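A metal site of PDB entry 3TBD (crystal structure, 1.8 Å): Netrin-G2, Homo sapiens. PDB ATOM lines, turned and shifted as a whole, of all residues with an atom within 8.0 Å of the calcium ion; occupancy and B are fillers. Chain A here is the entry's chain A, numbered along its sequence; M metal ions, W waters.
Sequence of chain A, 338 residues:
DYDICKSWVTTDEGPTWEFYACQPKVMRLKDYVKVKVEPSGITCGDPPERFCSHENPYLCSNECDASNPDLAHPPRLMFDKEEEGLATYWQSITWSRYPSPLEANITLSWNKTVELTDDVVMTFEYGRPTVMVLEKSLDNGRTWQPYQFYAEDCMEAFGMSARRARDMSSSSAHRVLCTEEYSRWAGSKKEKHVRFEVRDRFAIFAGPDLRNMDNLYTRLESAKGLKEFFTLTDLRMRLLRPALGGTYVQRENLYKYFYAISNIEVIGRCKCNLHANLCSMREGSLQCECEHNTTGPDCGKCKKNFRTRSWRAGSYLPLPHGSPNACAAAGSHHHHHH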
ATOM      1  N   LYS A  30      -2.017   8.490  30.082  1.00  0.00           N
ATOM      2  CA  LYS A  30      -1.096   9.650  30.210  1.00  0.00           C
ATOM      3  C   LYS A  30      -1.484  10.842  29.328  1.00  0.00           C
ATOM      4  O   LYS A  30      -1.048  11.964  29.613  1.00  0.00           O
ATOM      5  CB  LYS A  30       0.368   9.257  29.923  1.00  0.00           C
ATOM      6  CG  LYS A  30       0.624   9.086  28.442  1.00  0.00           C
ATOM      7  CD  LYS A  30       2.094   8.480  28.304  1.00  0.00           C
ATOM      8  CE  LYS A  30       2.560   8.569  26.860  1.00  0.00           C
ATOM      9  NZ  LYS A  30       3.873   7.672  26.687  1.00  0.00           N
ATOM     10  N   PRO A  74      11.002  20.092  32.251  1.00  0.00           N
ATOM     11  CA  PRO A  74       9.753  20.275  32.972  1.00  0.00           C
ATOM     12  C   PRO A  74       8.934  18.958  33.058  1.00  0.00           C
ATOM     13  O   PRO A  74       9.165  18.029  32.265  1.00  0.00           O
ATOM     14  CB  PRO A  74       9.006  21.288  32.118  1.00  0.00           C
ATOM     15  CG  PRO A  74       9.495  21.019  30.655  1.00  0.00           C
ATOM     16  CD  PRO A  74      10.987  20.730  30.915  1.00  0.00           C
ATOM     17  N   PRO A  75       7.972  18.916  33.946  1.00  0.00           N
ATOM     18  CA  PRO A  75       7.206  17.669  34.186  1.00  0.00           C
ATOM     19  C   PRO A  75       6.495  17.146  32.944  1.00  0.00           C
ATOM     20  O   PRO A  75       6.327  15.904  32.829  1.00  0.00           O
ATOM     21  CB  PRO A  75       6.157  18.124  35.202  1.00  0.00           C
ATOM     22  CG  PRO A  75       6.962  19.229  36.048  1.00  0.00           C
ATOM     23  CD  PRO A  75       7.686  19.955  34.977  1.00  0.00           C
ATOM     24  N   ARG A  76       6.084  18.011  31.999  1.00  0.00           N
ATOM     25  CA  ARG A  76       5.340  17.495  30.863  1.00  0.00           C
ATOM     26  C   ARG A  76       6.154  16.495  29.996  1.00  0.00           C
ATOM     27  O   ARG A  76       5.584  15.756  29.214  1.00  0.00           O
ATOM     28  CB  ARG A  76       4.794  18.650  29.983  1.00  0.00           C
ATOM     29  CG  ARG A  76       5.866  19.614  29.529  1.00  0.00           C
ATOM     30  CD  ARG A  76       5.187  20.786  28.787  1.00  0.00           C
ATOM     31  NE  ARG A  76       6.156  21.831  28.452  1.00  0.00           N
ATOM     32  CZ  ARG A  76       7.015  21.774  27.441  1.00  0.00           C
ATOM     33  NH1 ARG A  76       7.075  20.697  26.662  1.00  0.00           N
ATOM     34  NH2 ARG A  76       7.839  22.796  27.241  1.00  0.00           N
ATOM     35  N   LEU A  77       7.496  16.541  30.059  1.00  0.00           N
ATOM     36  CA  LEU A  77       8.307  15.571  29.330  1.00  0.00           C
ATOM     37  C   LEU A  77       8.085  14.126  29.821  1.00  0.00           C
ATOM     38  O   LEU A  77       8.591  13.237  29.181  1.00  0.00           O
ATOM     39  CB  LEU A  77       9.802  15.882  29.472  1.00  0.00           C
ATOM     40  CG  LEU A  77      10.074  17.307  28.869  1.00  0.00           C
ATOM     41  CD1 LEU A  77      11.624  17.486  28.893  1.00  0.00           C
ATOM     42  CD2 LEU A  77       9.470  17.399  27.433  1.00  0.00           C
ATOM     43  N   MET A  78       7.376  13.911  30.914  1.00  0.00           N
ATOM     44  CA  MET A  78       7.142  12.534  31.385  1.00  0.00           C
ATOM     45  C   MET A  78       6.032  11.867  30.510  1.00  0.00           C
ATOM     46  O   MET A  78       5.788  10.655  30.690  1.00  0.00           O
ATOM     47  CB  MET A  78       6.714  12.517  32.899  1.00  0.00           C
ATOM     48  CG  MET A  78       7.913  12.977  33.738  1.00  0.00           C
ATOM     49  SD  MET A  78       7.566  12.736  35.484  1.00  0.00           S
ATOM     50  CE  MET A  78       6.671  14.304  35.910  1.00  0.00           C
ATOM     51  N   PHE A  79       5.335  12.639  29.658  1.00  0.00           N
ATOM     52  CA  PHE A  79       4.108  12.116  29.019  1.00  0.00           C
ATOM     53  C   PHE A  79       4.082  12.293  27.489  1.00  0.00           C
ATOM     54  O   PHE A  79       3.012  12.032  26.874  1.00  0.00           O
ATOM     55  CB  PHE A  79       2.834  12.783  29.601  1.00  0.00           C
ATOM     56  CG  PHE A  79       2.835  12.804  31.072  1.00  0.00           C
ATOM     57  CD1 PHE A  79       2.770  11.575  31.805  1.00  0.00           C
ATOM     58  CD2 PHE A  79       3.068  14.029  31.756  1.00  0.00           C
ATOM     59  CE1 PHE A  79       2.837  11.616  33.222  1.00  0.00           C
ATOM     60  CE2 PHE A  79       3.172  14.105  33.102  1.00  0.00           C
ATOM     61  CZ  PHE A  79       3.044  12.892  33.912  1.00  0.00           C
ATOM     62  N   ASP A  80       5.163  12.840  26.943  1.00  0.00           N
ATOM     63  CA  ASP A  80       5.157  13.221  25.538  1.00  0.00           C
ATOM     64  C   ASP A  80       5.407  12.016  24.596  1.00  0.00           C
ATOM     65  O   ASP A  80       5.721  10.916  25.051  1.00  0.00           O
ATOM     66  CB  ASP A  80       6.143  14.313  25.242  1.00  0.00           C
ATOM     67  CG  ASP A  80       7.604  13.950  25.549  1.00  0.00           C
ATOM     68  OD1 ASP A  80       7.885  12.931  26.211  1.00  0.00           O
ATOM     69  OD2 ASP A  80       8.503  14.755  25.139  1.00  0.00           O
ATOM     70  N   LYS A  81       5.307  12.313  23.296  1.00  0.00           N
ATOM     71  CA  LYS A  81       5.700  11.306  22.291  1.00  0.00           C
ATOM     72  C   LYS A  81       7.149  11.498  22.008  1.00  0.00           C
ATOM     73  O   LYS A  81       7.560  12.651  21.772  1.00  0.00           O
ATOM     74  CB  LYS A  81       4.911  11.552  20.976  1.00  0.00           C
ATOM     75  CG  LYS A  81       3.482  10.968  21.059  1.00  0.00           C
ATOM     76  CD  LYS A  81       2.616  11.249  19.689  1.00  0.00           C
ATOM     77  CE  LYS A  81       1.423  12.250  19.893  1.00  0.00           C
ATOM     78  NZ  LYS A  81       0.421  12.054  18.731  1.00  0.00           N
ATOM     79  N   GLU A  82       7.921  10.422  21.971  1.00  0.00           N
ATOM     80  CA  GLU A  82       9.387  10.538  21.820  1.00  0.00           C
ATOM     81  C   GLU A  82       9.788   9.967  20.471  1.00  0.00           C
ATOM     82  O   GLU A  82       9.336   8.910  20.112  1.00  0.00           O
ATOM     83  CB  GLU A  82      10.168   9.816  22.916  1.00  0.00           C
ATOM     84  CG  GLU A  82       9.918  10.461  24.288  1.00  0.00           C
ATOM     85  CD  GLU A  82      10.607   9.739  25.411  1.00  0.00           C
ATOM     86  OE1 GLU A  82      10.899   8.553  25.326  1.00  0.00           O
ATOM     87  OE2 GLU A  82      10.897  10.363  26.491  1.00  0.00           O
ATOM     88  N   GLU A  83      10.601  10.727  19.775  1.00  0.00           N
ATOM     89  CA  GLU A  83      11.151  10.200  18.564  1.00  0.00           C
ATOM     90  C   GLU A  83      12.418   9.365  18.814  1.00  0.00           C
ATOM     91  O   GLU A  83      13.112   9.444  19.847  1.00  0.00           O
ATOM     92  CB  GLU A  83      11.318  11.321  17.512  1.00  0.00           C
ATOM     93  CG  GLU A  83      10.030  12.238  17.332  1.00  0.00           C
ATOM     94  CD  GLU A  83       8.752  11.513  16.896  1.00  0.00           C
ATOM     95  OE1 GLU A  83       8.796  10.732  15.902  1.00  0.00           O
ATOM     96  OE2 GLU A  83       7.667  11.695  17.560  1.00  0.00           O
ATOM     97  N   LEU A  86      15.844  10.058  21.039  1.00  0.00           N
ATOM     98  CA  LEU A  86      15.670  11.348  21.770  1.00  0.00           C
ATOM     99  C   LEU A  86      14.667  11.179  22.951  1.00  0.00           C
ATOM    100  O   LEU A  86      13.563  11.758  22.884  1.00  0.00           O
ATOM    101  CB  LEU A  86      15.263  12.464  20.808  1.00  0.00           C
ATOM    102  CG  LEU A  86      16.132  12.699  19.507  1.00  0.00           C
ATOM    103  CD1 LEU A  86      15.367  13.439  18.408  1.00  0.00           C
ATOM    104  CD2 LEU A  86      17.503  13.425  19.916  1.00  0.00           C
ATOM    105  N   ALA A  87      15.046  10.400  23.967  1.00  0.00           N
ATOM    106  CA  ALA A  87      14.245  10.385  25.242  1.00  0.00           C
ATOM    107  C   ALA A  87      14.183  11.801  25.800  1.00  0.00           C
ATOM    108  O   ALA A  87      15.180  12.588  25.684  1.00  0.00           O
ATOM    109  CB  ALA A  87      14.864   9.490  26.291  1.00  0.00           C
ATOM    110  N   THR A  88      13.054  12.163  26.377  1.00  0.00           N
ATOM    111  CA  THR A  88      12.922  13.511  27.003  1.00  0.00           C
ATOM    112  C   THR A  88      12.435  13.229  28.410  1.00  0.00           C
ATOM    113  O   THR A  88      11.580  12.339  28.613  1.00  0.00           O
ATOM    114  CB  THR A  88      11.854  14.368  26.324  1.00  0.00           C
ATOM    115  OG1 THR A  88      10.569  13.660  26.307  1.00  0.00           O
ATOM    116  CG2 THR A  88      12.274  14.674  24.880  1.00  0.00           C
ATOM    117  N   TYR A  89      12.966  13.975  29.363  1.00  0.00           N
ATOM    118  CA  TYR A  89      12.628  13.613  30.728  1.00  0.00           C
ATOM    119  C   TYR A  89      12.528  14.794  31.657  1.00  0.00           C
ATOM    120  O   TYR A  89      13.225  15.780  31.460  1.00  0.00           O
ATOM    121  CB  TYR A  89      13.628  12.630  31.296  1.00  0.00           C
ATOM    122  CG  TYR A  89      15.077  12.884  30.874  1.00  0.00           C
ATOM    123  CD1 TYR A  89      15.888  13.722  31.649  1.00  0.00           C
ATOM    124  CD2 TYR A  89      15.568  12.336  29.653  1.00  0.00           C
ATOM    125  CE1 TYR A  89      17.179  14.013  31.212  1.00  0.00           C
ATOM    126  CE2 TYR A  89      16.848  12.583  29.254  1.00  0.00           C
ATOM    127  CZ  TYR A  89      17.638  13.384  30.057  1.00  0.00           C
ATOM    128  OH  TYR A  89      18.938  13.610  29.577  1.00  0.00           O
ATOM    129  N   TRP A  90      11.675  14.640  32.659  1.00  0.00           N
ATOM    130  CA  TRP A  90      11.671  15.512  33.824  1.00  0.00           C
ATOM    131  C   TRP A  90      12.902  15.190  34.570  1.00  0.00           C
ATOM    132  O   TRP A  90      13.324  14.018  34.633  1.00  0.00           O
ATOM    133  CB  TRP A  90      10.371  15.305  34.681  1.00  0.00           C
ATOM    134  CG  TRP A  90      10.494  15.977  36.004  1.00  0.00           C
ATOM    135  CD1 TRP A  90      10.326  17.349  36.287  1.00  0.00           C
ATOM    136  CD2 TRP A  90      10.863  15.357  37.203  1.00  0.00           C
ATOM    137  NE1 TRP A  90      10.627  17.582  37.633  1.00  0.00           N
ATOM    138  CE2 TRP A  90      10.893  16.363  38.246  1.00  0.00           C
ATOM    139  CE3 TRP A  90      11.140  14.002  37.535  1.00  0.00           C
ATOM    140  CZ2 TRP A  90      11.231  16.050  39.583  1.00  0.00           C
ATOM    141  CZ3 TRP A  90      11.442  13.678  38.845  1.00  0.00           C
ATOM    142  CH2 TRP A  90      11.491  14.710  39.888  1.00  0.00           C
ATOM    143  N   THR A 123       9.496   5.026  33.775  1.00  0.00           N
ATOM    144  CA  THR A 123      10.839   4.804  33.225  1.00  0.00           C
ATOM    145  C   THR A 123      11.788   5.925  33.648  1.00  0.00           C
ATOM    146  O   THR A 123      11.546   7.097  33.296  1.00  0.00           O
ATOM    147  CB  THR A 123      10.719   4.829  31.648  1.00  0.00           C
ATOM    148  OG1 THR A 123       9.744   3.789  31.241  1.00  0.00           O
ATOM    149  CG2 THR A 123      12.176   4.629  30.962  1.00  0.00           C
ATOM    150  N   GLU A 125      15.692   7.582  33.772  1.00  0.00           N
ATOM    151  CA  GLU A 125      16.904   7.603  32.951  1.00  0.00           C
ATOM    152  C   GLU A 125      18.212   7.644  33.764  1.00  0.00           C
ATOM    153  O   GLU A 125      19.273   7.215  33.278  1.00  0.00           O
ATOM    154  CB  GLU A 125      16.896   8.864  32.078  1.00  0.00           C
ATOM    155  CG  GLU A 125      15.734   8.833  31.041  1.00  0.00           C
ATOM    156  CD  GLU A 125      15.810   7.640  30.106  1.00  0.00           C
ATOM    157  OE1 GLU A 125      16.935   7.252  29.754  1.00  0.00           O
ATOM    158  OE2 GLU A 125      14.739   7.094  29.720  1.00  0.00           O
ATOM    159  N   ILE A 261      12.838  11.209  34.942  1.00  0.00           N
ATOM    160  CA  ILE A 261      11.770  10.289  34.478  1.00  0.00           C
ATOM    161  C   ILE A 261      11.449  10.674  33.050  1.00  0.00           C
ATOM    162  O   ILE A 261      10.989  11.781  32.740  1.00  0.00           O
ATOM    163  CB  ILE A 261      10.524  10.413  35.359  1.00  0.00           C
ATOM    164  CG1 ILE A 261      10.886   9.988  36.795  1.00  0.00           C
ATOM    165  CG2 ILE A 261       9.308   9.488  34.738  1.00  0.00           C
ATOM    166  CD1 ILE A 261       9.729  10.361  37.830  1.00  0.00           C
ATOM    167  N   SER A 262      11.609   9.712  32.137  1.00  0.00           N
ATOM    168  CA  SER A 262      11.288  10.017  30.777  1.00  0.00           C
ATOM    169  C   SER A 262       9.913   9.654  30.325  1.00  0.00           C
ATOM    170  O   SER A 262       9.460  10.195  29.329  1.00  0.00           O
ATOM    171  CB  SER A 262      12.269   9.344  29.777  1.00  0.00           C
ATOM    172  OG  SER A 262      12.273   7.944  29.997  1.00  0.00           O
ATOM    173  N   ASN A 263       9.284   8.710  31.017  1.00  0.00           N
ATOM    174  CA  ASN A 263       7.942   8.321  30.547  1.00  0.00           C
ATOM    175  C   ASN A 263       7.184   7.634  31.695  1.00  0.00           C
ATOM    176  O   ASN A 263       7.785   6.811  32.471  1.00  0.00           O
ATOM    177  CB  ASN A 263       8.052   7.309  29.423  1.00  0.00           C
ATOM    178  CG  ASN A 263       6.709   7.139  28.690  1.00  0.00           C
ATOM    179  OD1 ASN A 263       6.191   8.056  28.099  1.00  0.00           O
ATOM    180  ND2 ASN A 263       6.123   5.926  28.791  1.00  0.00           N
ATOM    181  N   ILE A 264       5.878   7.969  31.809  1.00  0.00           N
ATOM    182  CA  ILE A 264       5.018   7.208  32.735  1.00  0.00           C
ATOM    183  C   ILE A 264       3.834   6.734  31.892  1.00  0.00           C
ATOM    184  O   ILE A 264       3.091   7.563  31.324  1.00  0.00           O
ATOM    185  CB  ILE A 264       4.492   8.089  33.902  1.00  0.00           C
ATOM    186  CG1 ILE A 264       5.733   8.549  34.732  1.00  0.00           C
ATOM    187  CG2 ILE A 264       3.570   7.205  34.793  1.00  0.00           C
ATOM    188  CD1 ILE A 264       5.322   9.647  35.810  1.00  0.00           C
HETATM  189 CA    CA M   1       9.461  11.805  27.581  1.00  0.00          CA
HETATM  190  O   HOH W   1       7.566  10.297  27.109  1.00  0.00           O
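Water W1 lies within hydrogen-bond range of OD1 of Asn 263 (2.8 Å) and O of Asp 80 (2.8 Å).
OE2 of Glu 82 binds the calcium ion (2.3 Å). The backbone carbonyl oxygen (O) of Leu 77 binds the calcium ion, 2.3 Å away. The calcium ion is bound by OD1 of Asp 80 (2.4 Å). O of Ser 262 is bound to the calcium ion (2.4 Å). O of Thr 88 binds the calcium ion, at 2.4 Å. Water W1 is bound to the calcium ion (2.5 Å). OG1 of Thr 88 is bound to the calcium ion (2.5 Å).
Within 4 Å of the calcium ion: Leu 77, Asp 80, Glu 82, Thr 88 and Ser 262. The nearest printed residue that does not touch the calcium ion is Met 78 (4.5 Å).
The backbone NH of Ser 262 lies within hydrogen-bond range of the backbone carbonyl oxygen of Thr 123, 2.9 Å away. The side-chain carboxylate (OE2) of Glu 125 is in hydrogen-bond range of the side-chain hydroxyl (OG) of Ser 262, 2.6 Å away.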
